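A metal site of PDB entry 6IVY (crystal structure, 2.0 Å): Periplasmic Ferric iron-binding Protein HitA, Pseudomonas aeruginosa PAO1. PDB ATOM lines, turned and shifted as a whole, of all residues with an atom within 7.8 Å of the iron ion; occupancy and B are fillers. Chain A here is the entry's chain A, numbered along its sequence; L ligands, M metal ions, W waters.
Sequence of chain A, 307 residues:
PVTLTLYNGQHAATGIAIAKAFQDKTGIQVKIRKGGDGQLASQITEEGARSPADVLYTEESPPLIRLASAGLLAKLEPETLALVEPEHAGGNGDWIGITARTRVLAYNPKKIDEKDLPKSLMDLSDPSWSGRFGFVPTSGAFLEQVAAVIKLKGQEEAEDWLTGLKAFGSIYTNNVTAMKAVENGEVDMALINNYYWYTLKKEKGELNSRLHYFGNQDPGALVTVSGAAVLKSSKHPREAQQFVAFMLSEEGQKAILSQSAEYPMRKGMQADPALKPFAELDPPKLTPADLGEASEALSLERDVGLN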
ATOM      1  N   GLY A   9      24.610  -2.084 -11.672  1.00  0.00           N
ATOM      2  CA  GLY A   9      23.686  -3.005 -11.037  1.00  0.00           C
ATOM      3  C   GLY A   9      22.977  -2.429  -9.828  1.00  0.00           C
ATOM      4  O   GLY A   9      22.001  -3.017  -9.364  1.00  0.00           O
ATOM      5  N   GLN A  10      23.486  -1.329  -9.273  1.00  0.00           N
ATOM      6  CA  GLN A  10      22.771  -0.724  -8.168  1.00  0.00           C
ATOM      7  C   GLN A  10      21.467  -0.131  -8.670  1.00  0.00           C
ATOM      8  O   GLN A  10      21.225  -0.006  -9.878  1.00  0.00           O
ATOM      9  CB  GLN A  10      23.618   0.342  -7.484  1.00  0.00           C
ATOM     10  CG  GLN A  10      24.204  -0.113  -6.148  1.00  0.00           C
ATOM     11  CD  GLN A  10      23.263   0.096  -4.967  1.00  0.00           C
ATOM     12  OE1 GLN A  10      22.040  -0.041  -5.090  1.00  0.00           O
ATOM     13  NE2 GLN A  10      23.825   0.441  -3.817  1.00  0.00           N
ATOM     14  N   HIS A  11      20.625   0.254  -7.720  1.00  0.00           N
ATOM     15  CA  HIS A  11      19.345   0.847  -8.067  1.00  0.00           C
ATOM     16  C   HIS A  11      19.555   2.099  -8.919  1.00  0.00           C
ATOM     17  O   HIS A  11      20.515   2.849  -8.712  1.00  0.00           O
ATOM     18  CB  HIS A  11      18.563   1.144  -6.801  1.00  0.00           C
ATOM     19  CG  HIS A  11      18.084  -0.103  -6.126  1.00  0.00           C
ATOM     20  ND1 HIS A  11      16.911  -0.740  -6.498  1.00  0.00           N
ATOM     21  CD2 HIS A  11      18.640  -0.877  -5.169  1.00  0.00           C
ATOM     22  CE1 HIS A  11      16.750  -1.829  -5.764  1.00  0.00           C
ATOM     23  NE2 HIS A  11      17.787  -1.937  -4.955  1.00  0.00           N
ATOM     24  N   ASP A  37      22.667  -7.163 -11.373  1.00  0.00           N
ATOM     25  CA  ASP A  37      24.063  -7.534 -11.080  1.00  0.00           C
ATOM     26  C   ASP A  37      24.522  -8.679 -11.988  1.00  0.00           C
ATOM     27  O   ASP A  37      25.496  -8.540 -12.756  1.00  0.00           O
ATOM     28  CB  ASP A  37      24.217  -7.963  -9.619  1.00  0.00           C
ATOM     29  CG  ASP A  37      24.161  -6.802  -8.624  1.00  0.00           C
ATOM     30  OD1 ASP A  37      24.144  -5.613  -9.022  1.00  0.00           O
ATOM     31  OD2 ASP A  37      24.137  -7.122  -7.403  1.00  0.00           O
ATOM     32  N   GLU A  59      24.945  -4.236  -6.567  1.00  0.00           N
ATOM     33  CA  GLU A  59      24.316  -4.250  -5.250  1.00  0.00           C
ATOM     34  C   GLU A  59      24.957  -5.260  -4.310  1.00  0.00           C
ATOM     35  O   GLU A  59      24.907  -5.082  -3.091  1.00  0.00           O
ATOM     36  CB  GLU A  59      22.831  -4.577  -5.388  1.00  0.00           C
ATOM     37  CG  GLU A  59      22.021  -3.507  -6.100  1.00  0.00           C
ATOM     38  CD  GLU A  59      20.531  -3.721  -5.936  1.00  0.00           C
ATOM     39  OE1 GLU A  59      20.070  -3.650  -4.786  1.00  0.00           O
ATOM     40  OE2 GLU A  59      19.844  -3.971  -6.954  1.00  0.00           O
ATOM     41  N   GLU A  60      25.563  -6.317  -4.851  1.00  0.00           N
ATOM     42  CA  GLU A  60      26.030  -7.440  -4.039  1.00  0.00           C
ATOM     43  C   GLU A  60      27.376  -7.915  -4.574  1.00  0.00           C
ATOM     44  O   GLU A  60      27.725  -7.638  -5.726  1.00  0.00           O
ATOM     45  CB  GLU A  60      25.031  -8.609  -4.065  1.00  0.00           C
ATOM     46  CG  GLU A  60      23.578  -8.172  -4.092  1.00  0.00           C
ATOM     47  CD  GLU A  60      23.113  -7.651  -2.732  1.00  0.00           C
ATOM     48  OE1 GLU A  60      22.077  -6.953  -2.662  1.00  0.00           O
ATOM     49  OE2 GLU A  60      23.784  -7.937  -1.725  1.00  0.00           O
ATOM     50  N   ARG A 101      24.541  -3.197   2.878  1.00  0.00           N
ATOM     51  CA  ARG A 101      23.115  -3.306   3.206  1.00  0.00           C
ATOM     52  C   ARG A 101      22.929  -4.500   4.128  1.00  0.00           C
ATOM     53  O   ARG A 101      23.838  -5.319   4.303  1.00  0.00           O
ATOM     54  CB  ARG A 101      22.252  -3.445   1.933  1.00  0.00           C
ATOM     55  CG  ARG A 101      22.701  -4.568   0.985  1.00  0.00           C
ATOM     56  CD  ARG A 101      23.673  -4.068  -0.110  1.00  0.00           C
ATOM     57  NE  ARG A 101      23.101  -3.015  -0.947  1.00  0.00           N
ATOM     58  CZ  ARG A 101      22.131  -3.208  -1.845  1.00  0.00           C
ATOM     59  NH1 ARG A 101      21.624  -4.413  -2.034  1.00  0.00           N
ATOM     60  NH2 ARG A 101      21.659  -2.179  -2.544  1.00  0.00           N
ATOM     61  N   SER A 139      16.230 -12.381  -5.888  1.00  0.00           N
ATOM     62  CA  SER A 139      16.992 -11.262  -5.351  1.00  0.00           C
ATOM     63  C   SER A 139      18.430 -11.657  -5.130  1.00  0.00           C
ATOM     64  O   SER A 139      18.726 -12.754  -4.659  1.00  0.00           O
ATOM     65  CB  SER A 139      16.375 -10.785  -4.039  1.00  0.00           C
ATOM     66  OG  SER A 139      17.341 -10.206  -3.203  1.00  0.00           O
ATOM     67  N   GLY A 140      19.338 -10.730  -5.447  1.00  0.00           N
ATOM     68  CA  GLY A 140      20.750 -10.983  -5.248  1.00  0.00           C
ATOM     69  C   GLY A 140      21.102 -11.157  -3.789  1.00  0.00           C
ATOM     70  O   GLY A 140      21.948 -11.992  -3.444  1.00  0.00           O
ATOM     71  N   ALA A 141      20.469 -10.380  -2.904  1.00  0.00           N
ATOM     72  CA  ALA A 141      20.773 -10.556  -1.480  1.00  0.00           C
ATOM     73  C   ALA A 141      20.093 -11.806  -0.917  1.00  0.00           C
ATOM     74  O   ALA A 141      20.600 -12.406   0.029  1.00  0.00           O
ATOM     75  CB  ALA A 141      20.383  -9.327  -0.665  1.00  0.00           C
ATOM     76  N   ASN A 174      10.381  -8.689  -6.676  1.00  0.00           N
ATOM     77  CA  ASN A 174      11.521  -7.895  -6.244  1.00  0.00           C
ATOM     78  C   ASN A 174      11.234  -7.403  -4.831  1.00  0.00           C
ATOM     79  O   ASN A 174      10.163  -7.660  -4.277  1.00  0.00           O
ATOM     80  CB  ASN A 174      11.800  -6.735  -7.211  1.00  0.00           C
ATOM     81  CG  ASN A 174      10.640  -5.759  -7.288  1.00  0.00           C
ATOM     82  OD1 ASN A 174      10.259  -5.164  -6.288  1.00  0.00           O
ATOM     83  ND2 ASN A 174      10.079  -5.577  -8.488  1.00  0.00           N
ATOM     84  N   ASN A 175      12.199  -6.714  -4.244  1.00  0.00           N
ATOM     85  CA  ASN A 175      12.052  -6.268  -2.859  1.00  0.00           C
ATOM     86  C   ASN A 175      11.067  -5.112  -2.751  1.00  0.00           C
ATOM     87  O   ASN A 175      10.467  -4.918  -1.690  1.00  0.00           O
ATOM     88  CB  ASN A 175      13.391  -5.844  -2.280  1.00  0.00           C
ATOM     89  CG  ASN A 175      14.345  -7.007  -2.081  1.00  0.00           C
ATOM     90  OD1 ASN A 175      13.971  -8.029  -1.469  1.00  0.00           O
ATOM     91  ND2 ASN A 175      15.591  -6.865  -2.569  1.00  0.00           N
ATOM     92  N   VAL A 176      10.913  -4.324  -3.824  1.00  0.00           N
ATOM     93  CA  VAL A 176      10.001  -3.193  -3.755  1.00  0.00           C
ATOM     94  C   VAL A 176       8.566  -3.684  -3.612  1.00  0.00           C
ATOM     95  O   VAL A 176       7.809  -3.184  -2.777  1.00  0.00           O
ATOM     96  CB  VAL A 176      10.176  -2.279  -4.975  1.00  0.00           C
ATOM     97  CG1 VAL A 176       9.222  -1.080  -4.878  1.00  0.00           C
ATOM     98  CG2 VAL A 176      11.626  -1.805  -5.082  1.00  0.00           C
ATOM     99  N   ASN A 193      15.845  -6.166   2.056  1.00  0.00           N
ATOM    100  CA  ASN A 193      16.977  -5.426   2.586  1.00  0.00           C
ATOM    101  C   ASN A 193      16.483  -4.180   3.327  1.00  0.00           C
ATOM    102  O   ASN A 193      15.353  -3.716   3.112  1.00  0.00           O
ATOM    103  CB  ASN A 193      17.962  -5.022   1.476  1.00  0.00           C
ATOM    104  CG  ASN A 193      18.509  -6.219   0.737  1.00  0.00           C
ATOM    105  OD1 ASN A 193      18.697  -7.301   1.327  1.00  0.00           O
ATOM    106  ND2 ASN A 193      18.746  -6.052  -0.564  1.00  0.00           N
ATOM    107  N   TYR A 195      17.171  -0.966   3.288  1.00  0.00           N
ATOM    108  CA  TYR A 195      17.024   0.372   2.727  1.00  0.00           C
ATOM    109  C   TYR A 195      15.669   0.599   2.066  1.00  0.00           C
ATOM    110  O   TYR A 195      15.253   1.743   1.901  1.00  0.00           O
ATOM    111  CB  TYR A 195      18.160   0.650   1.735  1.00  0.00           C
ATOM    112  CG  TYR A 195      18.328  -0.385   0.631  1.00  0.00           C
ATOM    113  CD1 TYR A 195      17.615  -0.264  -0.562  1.00  0.00           C
ATOM    114  CD2 TYR A 195      19.191  -1.479   0.788  1.00  0.00           C
ATOM    115  CE1 TYR A 195      17.754  -1.209  -1.582  1.00  0.00           C
ATOM    116  CE2 TYR A 195      19.334  -2.420  -0.223  1.00  0.00           C
ATOM    117  CZ  TYR A 195      18.603  -2.276  -1.393  1.00  0.00           C
ATOM    118  OH  TYR A 195      18.725  -3.211  -2.384  1.00  0.00           O
ATOM    119  N   TYR A 196      14.969  -0.475   1.718  1.00  0.00           N
ATOM    120  CA  TYR A 196      13.718  -0.325   0.977  1.00  0.00           C
ATOM    121  C   TYR A 196      12.649   0.378   1.803  1.00  0.00           C
ATOM    122  O   TYR A 196      11.841   1.135   1.268  1.00  0.00           O
ATOM    123  CB  TYR A 196      13.227  -1.689   0.522  1.00  0.00           C
ATOM    124  CG  TYR A 196      14.028  -2.293  -0.616  1.00  0.00           C
ATOM    125  CD1 TYR A 196      13.847  -1.857  -1.935  1.00  0.00           C
ATOM    126  CD2 TYR A 196      14.944  -3.302  -0.365  1.00  0.00           C
ATOM    127  CE1 TYR A 196      14.582  -2.420  -2.972  1.00  0.00           C
ATOM    128  CE2 TYR A 196      15.688  -3.858  -1.386  1.00  0.00           C
ATOM    129  CZ  TYR A 196      15.492  -3.424  -2.685  1.00  0.00           C
ATOM    130  OH  TYR A 196      16.207  -4.006  -3.693  1.00  0.00           O
ATOM    131  N   SER A 260      20.296   5.997  -1.234  1.00  0.00           N
ATOM    132  CA  SER A 260      20.105   4.670  -0.661  1.00  0.00           C
ATOM    133  C   SER A 260      20.494   4.708   0.811  1.00  0.00           C
ATOM    134  O   SER A 260      21.571   5.188   1.165  1.00  0.00           O
ATOM    135  CB  SER A 260      20.935   3.616  -1.413  1.00  0.00           C
ATOM    136  OG  SER A 260      20.262   2.363  -1.342  1.00  0.00           O
ATOM    137  N   GLU A 262      21.993   3.041   3.163  1.00  0.00           N
ATOM    138  CA  GLU A 262      22.970   1.983   3.355  1.00  0.00           C
ATOM    139  C   GLU A 262      24.086   2.434   4.287  1.00  0.00           C
ATOM    140  O   GLU A 262      24.121   3.591   4.736  1.00  0.00           O
ATOM    141  CB  GLU A 262      23.515   1.523   2.001  1.00  0.00           C
ATOM    142  CG  GLU A 262      22.443   0.886   1.171  1.00  0.00           C
ATOM    143  CD  GLU A 262      22.931   0.258  -0.096  1.00  0.00           C
ATOM    144  OE1 GLU A 262      23.978  -0.421  -0.097  1.00  0.00           O
ATOM    145  OE2 GLU A 262      22.244   0.447  -1.116  1.00  0.00           O
HETATM  146  P1  LIG L   1      18.811  -7.136  -4.142  1.00  0.00           P
HETATM  147  O1  LIG L   1      20.278  -7.284  -4.575  1.00  0.00           O
HETATM  148  O2  LIG L   1      18.551  -5.750  -3.638  1.00  0.00           O
HETATM  149  O3  LIG L   1      17.931  -7.376  -5.341  1.00  0.00           O
HETATM  150  O4  LIG L   1      18.501  -8.128  -3.025  1.00  0.00           O
HETATM  151 FE    FE M   1      18.128  -3.890  -3.952  1.00  0.00          FE
HETATM  152  O   HOH W   1      17.591  -4.777  -5.918  1.00  0.00           O
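The side-chain hydroxyl (OH) of Tyr 195 sits close to the guanidinium group (NH2) of Arg 101.
The side-chain amide nitrogen (ND2) of Asn 193 lies close to the side-chain hydroxyl (OH) of Tyr 195 (3.4 Å).
ND2 of Asn 175 lies close to OH of Tyr 196.
O of Glu 59 sits close to NE of Arg 101 (3.5 Å).
The side-chain carboxylate (OD1) of Asp 37 is in hydrogen-bond range of the backbone NH (N) of Glu 59, 2.9 Å away.
The iron ion is bound by OH of Tyr 195 (1.8 Å).
The iron ion is bound by O2 of the ligand, 1.9 Å away.
The side-chain hydroxyl (OH) of Tyr 196 binds the iron ion, at 1.9 Å.
The iron ion is bound by OE1 of Glu 59, 2.1 Å away.
The iron ion is bound by NE2 of His 11 (2.2 Å).
The iron ion is bound by water W1 (2.2 Å).
Of the 18 residues printed, 4 come within 4 Å of the iron ion.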
